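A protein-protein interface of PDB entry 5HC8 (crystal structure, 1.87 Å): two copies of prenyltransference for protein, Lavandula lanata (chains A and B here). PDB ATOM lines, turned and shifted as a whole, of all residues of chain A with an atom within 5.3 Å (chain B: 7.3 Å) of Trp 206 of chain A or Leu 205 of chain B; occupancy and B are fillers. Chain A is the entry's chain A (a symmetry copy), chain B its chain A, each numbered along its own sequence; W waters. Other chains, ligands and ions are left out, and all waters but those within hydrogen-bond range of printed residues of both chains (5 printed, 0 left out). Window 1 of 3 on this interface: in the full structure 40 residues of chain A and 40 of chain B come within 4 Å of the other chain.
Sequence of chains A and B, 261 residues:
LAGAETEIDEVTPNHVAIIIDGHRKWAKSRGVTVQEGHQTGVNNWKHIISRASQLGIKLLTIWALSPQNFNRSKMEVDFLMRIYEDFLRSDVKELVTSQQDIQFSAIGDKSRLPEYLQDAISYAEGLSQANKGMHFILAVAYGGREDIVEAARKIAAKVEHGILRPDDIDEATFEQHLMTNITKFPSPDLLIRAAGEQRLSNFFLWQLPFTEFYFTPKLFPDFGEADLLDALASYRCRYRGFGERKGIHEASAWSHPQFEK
OE1 of Glu 171 of chain A lies within salt-bridge range of NH1 of Arg 145 of chain B (2.8 Å).
OE1 of Glu 175 of chain A lies within salt-bridge range of NH2 of Arg 145 of chain B (3.7 Å).
The guanidinium group (NE) of Arg 145 of chain B sits at hydrogen-bond distance from the backbone carbonyl oxygen (O) of Trp 206 of chain A.
N of Ser 201 of chain B is in hydrogen-bond range of O of Pro 209 of chain A (2.8 Å).
The backbone carbonyl oxygen of Pro 209 of chain A lies within hydrogen-bond range of the backbone NH of Asn 202 of chain B, 2.9 Å away.
The backbone NH (N) of Gly 144 of chain B sits at hydrogen-bond distance from the backbone carbonyl oxygen (O) of Asn 202 of chain B (2.8 Å).
The backbone NH (N) of Arg 145 of chain B is in hydrogen-bond range of the side-chain amide oxygen (OD1) of Asn 202 of chain B.
ND2 of Asn 202 of chain B lies within hydrogen-bond range of OE1 of Glu 146 of chain B, at 2.9 Å.
OE1 of Glu 175 of chain A sits at hydrogen-bond distance from NE1 of Trp 206 of chain A, 3.0 Å away.
Among the printed residues, merely in contact across the chains: Ile 148 of chain A with Trp 206 of chain B (3.7 Å), Glu 171 of chain A with Val 149 of chain B (3.9 Å), Phe 174 of chain A with Ala 152 of chain B (3.6 Å), Leu 205 of chain A with Leu 205 of chain B (3.6 Å), Leu 205 of chain A with Trp 206 of chain B (3.9 Å), Leu 205 of chain A with Pro 209 of chain B (3.9 Å), Trp 206 of chain A with Ile 148 of chain B (3.7 Å), Trp 206 of chain A with Val 149 of chain B (3.7 Å), Trp 206 of chain A with Leu 205 of chain B (3.9 Å), Leu 208 of chain A with Leu 200 of chain B (3.8 Å), Pro 209 of chain A with Arg 145 of chain B (3.5 Å), Pro 209 of chain A with Leu 200 of chain B (3.6 Å) and Pro 209 of chain A with Leu 205 of chain B (3.9 Å).
Printed residues of chain B within 4 Å of Ile 148 of chain A: Trp 206.
Of the printed residues of chain B, Glu 171 of chain A touches Arg 145 and Val 149.
Of chain B, only Arg 145 (2.7 Å), Ile 148 (3.7 Å), Val 149 (3.7 Å) and Leu 205 (3.9 Å) come within 4 Å of Trp 206 of chain A.
Of the printed residues of chain A, Leu 200 of chain B touches Leu 208 (3.8 Å) and Pro 209 (3.6 Å).
Leu 205 of chain B touches three residues of chain A.
Leu 208 of chain B touches none of the printed residues of chain A.
The nearest residue of chain A that does not touch Leu 205 of chain B is Leu 208 of chain A (4.2 Å).
The nearest printed residue of chain B that does not touch Ile 148 of chain A is Ile 148 of chain B (4.02 Å).
Of the 20 printed residues of chain B, 10 touch a printed residue of chain A.
Of the 11 printed residues of chain A, 8 touch a printed residue of chain B.
Hydrophobic or aromatic side chains of chain A within 4 Å of the printed part of chain B: Ile 148, Phe 174, Leu 205, Trp 206 and Pro 209.
Among the printed residues, Asp or Glu carboxylates within 4 Å of a Lys or Arg side-chain nitrogen of the other chain: Glu 171 of chain A with Arg 145 of chain B and Glu 175 of chain A with Arg 145 of chain B.
Ile 148 of chain A touches Trp 206 of chain B, and with the chains exchanged Trp 206 of chain A touches Ile 148 of chain B.
Leu 205 of chain A touches its own counterpart, Leu 205 of chain B.
Leu 205 of chain A touches Trp 206 of chain B, and with the chains exchanged Trp 206 of chain A touches Leu 205 of chain B.
Leu 205 of chain A touches Pro 209 of chain B, and with the chains exchanged Pro 209 of chain A touches Leu 205 of chain B.
Of the 18 pairs that touch across the chains among the printed residues, 7 have their exchanged pair printed and touching as well.
Water W2 bridges the side-chain carboxylate (OE1) of Glu 175 of chain A (2.7 Å) and the guanidinium group (NH2) of Arg 145 of chain B (3.0 Å).
Water W4 lies within hydrogen-bond range of O of Leu 208 of chain A, N of Leu 200 of chain B and O of Pro 209 of chain A.
Water W5 lies within hydrogen-bond range of OE2 of Glu 175 of chain A and NH2 of Arg 145 of chain B.
Water W3 bridges OE2 of Glu 171 of chain A and OE2 of Glu 146 of chain B.
Water W1 bridges the side-chain carboxylate (OE1) of Glu 175 of chain A (3.0 Å) and the guanidinium group (NH1) of Arg 145 of chain B (3.3 Å).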
ATOM      1  N   ILE A 148       1.163 -11.581 -23.857  1.00  0.00           N
ATOM      2  CA  ILE A 148       0.027 -11.139 -24.485  1.00  0.00           C
ATOM      3  C   ILE A 148      -0.048  -9.592 -24.530  1.00  0.00           C
ATOM      4  O   ILE A 148      -0.423  -8.992 -25.567  1.00  0.00           O
ATOM      5  CB  ILE A 148      -1.206 -11.726 -23.869  1.00  0.00           C
ATOM      6  CG1 ILE A 148      -1.218 -13.269 -24.106  1.00  0.00           C
ATOM      7  CG2 ILE A 148      -2.489 -11.076 -24.394  1.00  0.00           C
ATOM      8  CD1 ILE A 148      -2.253 -13.958 -23.233  1.00  0.00           C
ATOM      9  N   GLU A 171      -6.033 -14.589 -35.244  1.00  0.00           N
ATOM     10  CA  GLU A 171      -5.077 -15.392 -34.446  1.00  0.00           C
ATOM     11  C   GLU A 171      -3.683 -15.343 -34.942  1.00  0.00           C
ATOM     12  O   GLU A 171      -2.686 -15.229 -34.188  1.00  0.00           O
ATOM     13  CB  GLU A 171      -5.436 -16.891 -34.344  1.00  0.00           C
ATOM     14  CG  GLU A 171      -6.451 -17.174 -33.341  1.00  0.00           C
ATOM     15  CD  GLU A 171      -6.819 -18.635 -33.309  1.00  0.00           C
ATOM     16  OE1 GLU A 171      -6.015 -19.405 -32.832  1.00  0.00           O
ATOM     17  OE2 GLU A 171      -7.891 -19.000 -33.825  1.00  0.00           O
ATOM     18  N   PHE A 174      -1.835 -12.268 -34.271  1.00  0.00           N
ATOM     19  CA  PHE A 174      -1.551 -12.102 -32.848  1.00  0.00           C
ATOM     20  C   PHE A 174      -0.396 -12.988 -32.454  1.00  0.00           C
ATOM     21  O   PHE A 174       0.583 -12.549 -31.872  1.00  0.00           O
ATOM     22  CB  PHE A 174      -2.834 -12.298 -32.033  1.00  0.00           C
ATOM     23  CG  PHE A 174      -2.733 -11.697 -30.670  1.00  0.00           C
ATOM     24  CD1 PHE A 174      -2.060 -12.367 -29.682  1.00  0.00           C
ATOM     25  CD2 PHE A 174      -3.209 -10.420 -30.430  1.00  0.00           C
ATOM     26  CE1 PHE A 174      -1.914 -11.805 -28.433  1.00  0.00           C
ATOM     27  CE2 PHE A 174      -3.080  -9.847 -29.160  1.00  0.00           C
ATOM     28  CZ  PHE A 174      -2.377 -10.526 -28.191  1.00  0.00           C
ATOM     29  N   GLU A 175      -0.388 -14.192 -33.001  1.00  0.00           N
ATOM     30  CA  GLU A 175       0.669 -15.161 -32.798  1.00  0.00           C
ATOM     31  C   GLU A 175       2.034 -14.673 -33.243  1.00  0.00           C
ATOM     32  O   GLU A 175       3.044 -14.874 -32.580  1.00  0.00           O
ATOM     33  CB  GLU A 175       0.171 -16.418 -33.541  1.00  0.00           C
ATOM     34  CG  GLU A 175       0.913 -17.736 -33.574  1.00  0.00           C
ATOM     35  CD  GLU A 175       0.650 -18.565 -32.380  1.00  0.00           C
ATOM     36  OE1 GLU A 175      -0.428 -19.228 -32.215  1.00  0.00           O
ATOM     37  OE2 GLU A 175       1.581 -18.478 -31.573  1.00  0.00           O
ATOM     38  N   LEU A 178       3.933 -12.503 -30.472  1.00  0.00           N
ATOM     39  CA  LEU A 178       4.344 -13.034 -29.162  1.00  0.00           C
ATOM     40  C   LEU A 178       5.778 -13.345 -29.188  1.00  0.00           C
ATOM     41  O   LEU A 178       6.408 -13.417 -30.279  1.00  0.00           O
ATOM     42  CB  LEU A 178       3.530 -14.317 -28.843  1.00  0.00           C
ATOM     43  CG  LEU A 178       2.041 -13.996 -28.704  1.00  0.00           C
ATOM     44  CD1 LEU A 178       1.220 -15.267 -28.884  1.00  0.00           C
ATOM     45  CD2 LEU A 178       1.742 -13.424 -27.300  1.00  0.00           C
ATOM     46  N   PHE A 204       3.026 -19.646 -20.186  1.00  0.00           N
ATOM     47  CA  PHE A 204       2.199 -19.510 -21.361  1.00  0.00           C
ATOM     48  C   PHE A 204       0.721 -19.546 -21.066  1.00  0.00           C
ATOM     49  O   PHE A 204       0.203 -20.389 -20.293  1.00  0.00           O
ATOM     50  CB  PHE A 204       2.450 -20.699 -22.373  1.00  0.00           C
ATOM     51  CG  PHE A 204       3.822 -20.803 -22.975  1.00  0.00           C
ATOM     52  CD1 PHE A 204       4.551 -19.709 -23.377  1.00  0.00           C
ATOM     53  CD2 PHE A 204       4.381 -22.066 -23.204  1.00  0.00           C
ATOM     54  CE1 PHE A 204       5.806 -19.851 -23.908  1.00  0.00           C
ATOM     55  CE2 PHE A 204       5.658 -22.224 -23.788  1.00  0.00           C
ATOM     56  CZ  PHE A 204       6.379 -21.104 -24.169  1.00  0.00           C
ATOM     57  N   LEU A 205      -0.026 -18.710 -21.774  1.00  0.00           N
ATOM     58  CA  LEU A 205      -1.461 -18.707 -21.696  1.00  0.00           C
ATOM     59  C   LEU A 205      -1.981 -18.834 -23.126  1.00  0.00           C
ATOM     60  O   LEU A 205      -2.637 -19.805 -23.426  1.00  0.00           O
ATOM     61  CB  LEU A 205      -1.995 -17.404 -21.025  1.00  0.00           C
ATOM     62  CG  LEU A 205      -1.517 -17.251 -19.555  1.00  0.00           C
ATOM     63  CD1 LEU A 205      -1.998 -15.878 -19.038  1.00  0.00           C
ATOM     64  CD2 LEU A 205      -2.015 -18.328 -18.667  1.00  0.00           C
ATOM     65  N   TRP A 206      -1.713 -17.843 -24.014  1.00  0.00           N
ATOM     66  CA  TRP A 206      -2.118 -17.931 -25.402  1.00  0.00           C
ATOM     67  C   TRP A 206      -1.716 -19.295 -26.026  1.00  0.00           C
ATOM     68  O   TRP A 206      -2.480 -19.867 -26.834  1.00  0.00           O
ATOM     69  CB  TRP A 206      -1.481 -16.820 -26.216  1.00  0.00           C
ATOM     70  CG  TRP A 206      -1.653 -16.979 -27.689  1.00  0.00           C
ATOM     71  CD1 TRP A 206      -0.925 -17.768 -28.528  1.00  0.00           C
ATOM     72  CD2 TRP A 206      -2.694 -16.374 -28.486  1.00  0.00           C
ATOM     73  NE1 TRP A 206      -1.426 -17.664 -29.809  1.00  0.00           N
ATOM     74  CE2 TRP A 206      -2.520 -16.822 -29.808  1.00  0.00           C
ATOM     75  CE3 TRP A 206      -3.705 -15.461 -28.220  1.00  0.00           C
ATOM     76  CZ2 TRP A 206      -3.343 -16.378 -30.846  1.00  0.00           C
ATOM     77  CZ3 TRP A 206      -4.568 -15.113 -29.205  1.00  0.00           C
ATOM     78  CH2 TRP A 206      -4.344 -15.512 -30.533  1.00  0.00           C
ATOM     79  N   GLN A 207      -0.532 -19.726 -25.649  1.00  0.00           N
ATOM     80  CA  GLN A 207       0.078 -20.917 -26.212  1.00  0.00           C
ATOM     81  C   GLN A 207      -0.585 -22.234 -25.882  1.00  0.00           C
ATOM     82  O   GLN A 207      -0.230 -23.233 -26.534  1.00  0.00           O
ATOM     83  CB  GLN A 207       1.600 -20.955 -25.976  1.00  0.00           C
ATOM     84  CG  GLN A 207       2.384 -19.828 -26.639  1.00  0.00           C
ATOM     85  CD  GLN A 207       2.423 -18.479 -25.894  1.00  0.00           C
ATOM     86  OE1 GLN A 207       1.726 -18.273 -24.863  1.00  0.00           O
ATOM     87  NE2 GLN A 207       3.241 -17.547 -26.410  1.00  0.00           N
ATOM     88  N   LEU A 208      -1.519 -22.269 -24.943  1.00  0.00           N
ATOM     89  CA  LEU A 208      -1.981 -23.537 -24.322  1.00  0.00           C
ATOM     90  C   LEU A 208      -3.377 -24.065 -24.604  1.00  0.00           C
ATOM     91  O   LEU A 208      -3.834 -24.865 -23.805  1.00  0.00           O
ATOM     92  CB  LEU A 208      -1.792 -23.447 -22.760  1.00  0.00           C
ATOM     93  CG  LEU A 208      -0.376 -23.192 -22.251  1.00  0.00           C
ATOM     94  CD1 LEU A 208      -0.404 -23.388 -20.716  1.00  0.00           C
ATOM     95  CD2 LEU A 208       0.664 -24.149 -22.838  1.00  0.00           C
ATOM     96  N   PRO A 209      -4.101 -23.627 -25.704  1.00  0.00           N
ATOM     97  CA  PRO A 209      -5.514 -24.007 -25.845  1.00  0.00           C
ATOM     98  C   PRO A 209      -5.704 -25.524 -25.959  1.00  0.00           C
ATOM     99  O   PRO A 209      -6.675 -26.019 -25.422  1.00  0.00           O
ATOM    100  CB  PRO A 209      -5.989 -23.280 -27.140  1.00  0.00           C
ATOM    101  CG  PRO A 209      -4.733 -22.940 -27.886  1.00  0.00           C
ATOM    102  CD  PRO A 209      -3.640 -22.818 -26.849  1.00  0.00           C
ATOM    103  N   TYR B 142     -17.958 -19.638 -26.929  1.00  0.00           N
ATOM    104  CA  TYR B 142     -16.864 -18.918 -26.223  1.00  0.00           C
ATOM    105  C   TYR B 142     -15.594 -19.718 -26.422  1.00  0.00           C
ATOM    106  O   TYR B 142     -15.576 -20.969 -26.150  1.00  0.00           O
ATOM    107  CB  TYR B 142     -17.118 -18.832 -24.684  1.00  0.00           C
ATOM    108  CG  TYR B 142     -15.922 -18.182 -24.062  1.00  0.00           C
ATOM    109  CD1 TYR B 142     -15.778 -16.785 -24.093  1.00  0.00           C
ATOM    110  CD2 TYR B 142     -14.859 -18.947 -23.671  1.00  0.00           C
ATOM    111  CE1 TYR B 142     -14.631 -16.182 -23.655  1.00  0.00           C
ATOM    112  CE2 TYR B 142     -13.673 -18.382 -23.259  1.00  0.00           C
ATOM    113  CZ  TYR B 142     -13.600 -16.981 -23.187  1.00  0.00           C
ATOM    114  OH  TYR B 142     -12.400 -16.445 -22.860  1.00  0.00           O
ATOM    115  N   GLY B 143     -14.564 -19.069 -26.951  1.00  0.00           N
ATOM    116  CA  GLY B 143     -13.234 -19.661 -26.991  1.00  0.00           C
ATOM    117  C   GLY B 143     -12.212 -18.684 -26.464  1.00  0.00           C
ATOM    118  O   GLY B 143     -12.374 -17.474 -26.645  1.00  0.00           O
ATOM    119  N   GLY B 144     -11.191 -19.156 -25.748  1.00  0.00           N
ATOM    120  CA  GLY B 144     -10.214 -18.269 -25.123  1.00  0.00           C
ATOM    121  C   GLY B 144      -9.338 -17.476 -26.097  1.00  0.00           C
ATOM    122  O   GLY B 144      -9.078 -16.311 -25.878  1.00  0.00           O
ATOM    123  N   ARG B 145      -8.867 -18.125 -27.171  1.00  0.00           N
ATOM    124  CA  ARG B 145      -8.128 -17.447 -28.234  1.00  0.00           C
ATOM    125  C   ARG B 145      -9.017 -16.358 -28.860  1.00  0.00           C
ATOM    126  O   ARG B 145      -8.560 -15.254 -29.027  1.00  0.00           O
ATOM    127  CB  ARG B 145      -7.744 -18.424 -29.365  1.00  0.00           C
ATOM    128  CG  ARG B 145      -6.630 -19.369 -29.047  1.00  0.00           C
ATOM    129  CD  ARG B 145      -5.314 -18.717 -29.124  1.00  0.00           C
ATOM    130  NE  ARG B 145      -4.132 -19.592 -28.965  1.00  0.00           N
ATOM    131  CZ  ARG B 145      -3.479 -20.291 -29.899  1.00  0.00           C
ATOM    132  NH1 ARG B 145      -3.963 -20.423 -31.143  1.00  0.00           N
ATOM    133  NH2 ARG B 145      -2.371 -20.956 -29.565  1.00  0.00           N
ATOM    134  N   GLU B 146     -10.250 -16.702 -29.135  1.00  0.00           N
ATOM    135  CA  GLU B 146     -11.171 -15.772 -29.785  1.00  0.00           C
ATOM    136  C   GLU B 146     -11.431 -14.531 -28.914  1.00  0.00           C
ATOM    137  O   GLU B 146     -11.469 -13.393 -29.403  1.00  0.00           O
ATOM    138  CB  GLU B 146     -12.485 -16.409 -30.064  1.00  0.00           C
ATOM    139  CG  GLU B 146     -12.541 -17.367 -31.193  1.00  0.00           C
ATOM    140  CD  GLU B 146     -11.863 -18.718 -30.911  1.00  0.00           C
ATOM    141  OE1 GLU B 146     -11.409 -19.024 -29.776  1.00  0.00           O
ATOM    142  OE2 GLU B 146     -11.841 -19.524 -31.863  1.00  0.00           O
ATOM    143  N   ASP B 147     -11.597 -14.761 -27.610  1.00  0.00           N
ATOM    144  CA  ASP B 147     -11.647 -13.674 -26.620  1.00  0.00           C
ATOM    145  C   ASP B 147     -10.462 -12.723 -26.682  1.00  0.00           C
ATOM    146  O   ASP B 147     -10.630 -11.489 -26.717  1.00  0.00           O
ATOM    147  CB  ASP B 147     -11.783 -14.303 -25.214  1.00  0.00           C
ATOM    148  CG  ASP B 147     -12.350 -13.383 -24.176  1.00  0.00           C
ATOM    149  OD1 ASP B 147     -12.875 -12.242 -24.467  1.00  0.00           O
ATOM    150  OD2 ASP B 147     -12.313 -13.871 -22.994  1.00  0.00           O
ATOM    151  N   ILE B 148      -9.232 -13.234 -26.617  1.00  0.00           N
ATOM    152  CA  ILE B 148      -8.100 -12.463 -26.697  1.00  0.00           C
ATOM    153  C   ILE B 148      -8.035 -11.664 -28.023  1.00  0.00           C
ATOM    154  O   ILE B 148      -7.667 -10.464 -28.038  1.00  0.00           O
ATOM    155  CB  ILE B 148      -6.862 -13.281 -26.492  1.00  0.00           C
ATOM    156  CG1 ILE B 148      -6.841 -13.832 -25.031  1.00  0.00           C
ATOM    157  CG2 ILE B 148      -5.585 -12.497 -26.805  1.00  0.00           C
ATOM    158  CD1 ILE B 148      -5.799 -14.925 -24.863  1.00  0.00           C
ATOM    159  N   VAL B 149      -8.331 -12.285 -29.125  1.00  0.00           N
ATOM    160  CA  VAL B 149      -8.215 -11.591 -30.436  1.00  0.00           C
ATOM    161  C   VAL B 149      -9.237 -10.455 -30.499  1.00  0.00           C
ATOM    162  O   VAL B 149      -8.908  -9.357 -30.904  1.00  0.00           O
ATOM    163  CB  VAL B 149      -8.428 -12.571 -31.610  1.00  0.00           C
ATOM    164  CG1 VAL B 149      -8.538 -11.823 -32.952  1.00  0.00           C
ATOM    165  CG2 VAL B 149      -7.301 -13.591 -31.707  1.00  0.00           C
ATOM    166  N   ALA B 152      -8.096  -7.634 -28.456  1.00  0.00           N
ATOM    167  CA  ALA B 152      -7.057  -6.996 -29.242  1.00  0.00           C
ATOM    168  C   ALA B 152      -7.649  -6.067 -30.364  1.00  0.00           C
ATOM    169  O   ALA B 152      -7.160  -4.921 -30.544  1.00  0.00           O
ATOM    170  CB  ALA B 152      -6.078  -8.023 -29.789  1.00  0.00           C
ATOM    171  N   LEU B 200      -7.225 -27.607 -21.673  1.00  0.00           N
ATOM    172  CA  LEU B 200      -8.165 -26.489 -21.658  1.00  0.00           C
ATOM    173  C   LEU B 200      -9.102 -26.503 -22.826  1.00  0.00           C
ATOM    174  O   LEU B 200     -10.205 -25.923 -22.736  1.00  0.00           O
ATOM    175  CB  LEU B 200      -7.369 -25.171 -21.610  1.00  0.00           C
ATOM    176  CG  LEU B 200      -6.404 -25.070 -20.410  1.00  0.00           C
ATOM    177  CD1 LEU B 200      -5.587 -23.783 -20.577  1.00  0.00           C
ATOM    178  CD2 LEU B 200      -7.160 -25.041 -19.086  1.00  0.00           C
ATOM    179  N   SER B 201      -8.706 -27.139 -23.935  1.00  0.00           N
ATOM    180  CA  SER B 201      -9.587 -27.169 -25.113  1.00  0.00           C
ATOM    181  C   SER B 201     -10.129 -25.822 -25.595  1.00  0.00           C
ATOM    182  O   SER B 201     -11.239 -25.722 -26.118  1.00  0.00           O
ATOM    183  CB  SER B 201     -10.751 -28.155 -24.933  1.00  0.00           C
ATOM    184  OG  SER B 201     -10.252 -29.405 -24.506  1.00  0.00           O
ATOM    185  N   ASN B 202      -9.322 -24.788 -25.425  1.00  0.00           N
ATOM    186  CA  ASN B 202      -9.582 -23.436 -25.883  1.00  0.00           C
ATOM    187  C   ASN B 202     -10.702 -22.779 -25.075  1.00  0.00           C
ATOM    188  O   ASN B 202     -11.494 -21.940 -25.565  1.00  0.00           O
ATOM    189  CB  ASN B 202      -9.716 -23.337 -27.424  1.00  0.00           C
ATOM    190  CG  ASN B 202      -9.798 -21.917 -27.892  1.00  0.00           C
ATOM    191  OD1 ASN B 202      -9.067 -21.054 -27.423  1.00  0.00           O
ATOM    192  ND2 ASN B 202     -10.737 -21.645 -28.774  1.00  0.00           N
ATOM    193  N   PHE B 203     -10.769 -23.158 -23.787  1.00  0.00           N
ATOM    194  CA  PHE B 203     -11.501 -22.329 -22.824  1.00  0.00           C
ATOM    195  C   PHE B 203     -10.712 -21.049 -22.516  1.00  0.00           C
ATOM    196  O   PHE B 203      -9.825 -20.604 -23.288  1.00  0.00           O
ATOM    197  CB  PHE B 203     -11.845 -23.182 -21.576  1.00  0.00           C
ATOM    198  CG  PHE B 203     -12.850 -22.590 -20.602  1.00  0.00           C
ATOM    199  CD1 PHE B 203     -13.992 -21.867 -20.993  1.00  0.00           C
ATOM    200  CD2 PHE B 203     -12.697 -22.878 -19.245  1.00  0.00           C
ATOM    201  CE1 PHE B 203     -14.872 -21.343 -20.091  1.00  0.00           C
ATOM    202  CE2 PHE B 203     -13.608 -22.365 -18.300  1.00  0.00           C
ATOM    203  CZ  PHE B 203     -14.724 -21.625 -18.723  1.00  0.00           C
ATOM    204  N   PHE B 204     -11.035 -20.401 -21.384  1.00  0.00           N
ATOM    205  CA  PHE B 204     -10.213 -19.306 -20.929  1.00  0.00           C
ATOM    206  C   PHE B 204      -8.734 -19.572 -21.047  1.00  0.00           C
ATOM    207  O   PHE B 204      -8.208 -20.656 -20.694  1.00  0.00           O
ATOM    208  CB  PHE B 204     -10.460 -19.009 -19.396  1.00  0.00           C
ATOM    209  CG  PHE B 204     -11.834 -18.543 -19.005  1.00  0.00           C
ATOM    210  CD1 PHE B 204     -12.570 -17.661 -19.759  1.00  0.00           C
ATOM    211  CD2 PHE B 204     -12.387 -18.967 -17.790  1.00  0.00           C
ATOM    212  CE1 PHE B 204     -13.826 -17.275 -19.370  1.00  0.00           C
ATOM    213  CE2 PHE B 204     -13.664 -18.543 -17.362  1.00  0.00           C
ATOM    214  CZ  PHE B 204     -14.393 -17.666 -18.148  1.00  0.00           C
ATOM    215  N   LEU B 205      -7.994 -18.541 -21.432  1.00  0.00           N
ATOM    216  CA  LEU B 205      -6.559 -18.598 -21.477  1.00  0.00           C
ATOM    217  C   LEU B 205      -6.043 -17.413 -20.666  1.00  0.00           C
ATOM    218  O   LEU B 205      -5.383 -17.623 -19.676  1.00  0.00           O
ATOM    219  CB  LEU B 205      -6.030 -18.541 -22.943  1.00  0.00           C
ATOM    220  CG  LEU B 205      -6.504 -19.749 -23.797  1.00  0.00           C
ATOM    221  CD1 LEU B 205      -6.030 -19.523 -25.249  1.00  0.00           C
ATOM    222  CD2 LEU B 205      -5.996 -21.048 -23.295  1.00  0.00           C
ATOM    223  N   TRP B 206      -6.319 -16.154 -21.092  1.00  0.00           N
ATOM    224  CA  TRP B 206      -5.919 -14.985 -20.336  1.00  0.00           C
ATOM    225  C   TRP B 206      -6.315 -15.113 -18.841  1.00  0.00           C
ATOM    226  O   TRP B 206      -5.551 -14.686 -17.948  1.00  0.00           O
ATOM    227  CB  TRP B 206      -6.565 -13.734 -20.903  1.00  0.00           C
ATOM    228  CG  TRP B 206      -6.397 -12.527 -20.042  1.00  0.00           C
ATOM    229  CD1 TRP B 206      -7.123 -12.189 -18.940  1.00  0.00           C
ATOM    230  CD2 TRP B 206      -5.362 -11.531 -20.181  1.00  0.00           C
ATOM    231  NE1 TRP B 206      -6.627 -11.019 -18.404  1.00  0.00           N
ATOM    232  CE2 TRP B 206      -5.539 -10.600 -19.142  1.00  0.00           C
ATOM    233  CE3 TRP B 206      -4.356 -11.308 -21.111  1.00  0.00           C
ATOM    234  CZ2 TRP B 206      -4.721  -9.472 -19.022  1.00  0.00           C
ATOM    235  CZ3 TRP B 206      -3.498 -10.275 -20.933  1.00  0.00           C
ATOM    236  CH2 TRP B 206      -3.725  -9.314 -19.933  1.00  0.00           C
ATOM    237  N   GLN B 207      -7.495 -15.660 -18.646  1.00  0.00           N
ATOM    238  CA  GLN B 207      -8.100 -15.758 -17.330  1.00  0.00           C
ATOM    239  C   GLN B 207      -7.429 -16.688 -16.347  1.00  0.00           C
ATOM    240  O   GLN B 207      -7.780 -16.612 -15.155  1.00  0.00           O
ATOM    241  CB  GLN B 207      -9.621 -15.991 -17.407  1.00  0.00           C
ATOM    242  CG  GLN B 207     -10.415 -14.865 -18.061  1.00  0.00           C
ATOM    243  CD  GLN B 207     -10.458 -14.852 -19.602  1.00  0.00           C
ATOM    244  OE1 GLN B 207      -9.759 -15.645 -20.290  1.00  0.00           O
ATOM    245  NE2 GLN B 207     -11.283 -13.949 -20.158  1.00  0.00           N
ATOM    246  N   LEU B 208      -6.491 -17.517 -16.779  1.00  0.00           N
ATOM    247  CA  LEU B 208      -6.020 -18.678 -15.982  1.00  0.00           C
ATOM    248  C   LEU B 208      -4.622 -18.683 -15.388  1.00  0.00           C
ATOM    249  O   LEU B 208      -4.158 -19.769 -15.085  1.00  0.00           O
ATOM    250  CB  LEU B 208      -6.204 -19.996 -16.826  1.00  0.00           C
ATOM    251  CG  LEU B 208      -7.619 -20.322 -17.292  1.00  0.00           C
ATOM    252  CD1 LEU B 208      -7.585 -21.755 -17.876  1.00  0.00           C
ATOM    253  CD2 LEU B 208      -8.656 -20.286 -16.168  1.00  0.00           C
ATOM    254  N   PRO B 209      -3.904 -17.505 -15.232  1.00  0.00           N
ATOM    255  CA  PRO B 209      -2.489 -17.561 -14.836  1.00  0.00           C
ATOM    256  C   PRO B 209      -2.291 -18.205 -13.460  1.00  0.00           C
ATOM    257  O   PRO B 209      -1.315 -18.910 -13.295  1.00  0.00           O
ATOM    258  CB  PRO B 209      -2.023 -16.073 -14.836  1.00  0.00           C
ATOM    259  CG  PRO B 209      -3.283 -15.264 -14.762  1.00  0.00           C
ATOM    260  CD  PRO B 209      -4.373 -16.114 -15.373  1.00  0.00           C
ATOM    261  N   THR B 211      -5.209 -19.717 -11.577  1.00  0.00           N
ATOM    262  CA  THR B 211      -6.243 -20.671 -11.311  1.00  0.00           C
ATOM    263  C   THR B 211      -5.745 -22.093 -10.910  1.00  0.00           C
ATOM    264  O   THR B 211      -4.817 -22.663 -11.483  1.00  0.00           O
ATOM    265  CB  THR B 211      -7.057 -20.817 -12.589  1.00  0.00           C
ATOM    266  OG1 THR B 211      -7.454 -19.504 -13.038  1.00  0.00           O
ATOM    267  CG2 THR B 211      -8.256 -21.721 -12.398  1.00  0.00           C
HETATM  268  O   HOH W   1      -2.695 -19.760 -34.148  1.00  0.00           O
HETATM  269  O   HOH W   2      -1.162 -21.784 -32.239  1.00  0.00           O
HETATM  270  O   HOH W   3      -8.998 -21.063 -32.077  1.00  0.00           O
HETATM  271  O   HOH W   4      -4.735 -27.281 -22.965  1.00  0.00           O
HETATM  272  O   HOH W   5       0.890 -20.439 -29.625  1.00  0.00           O
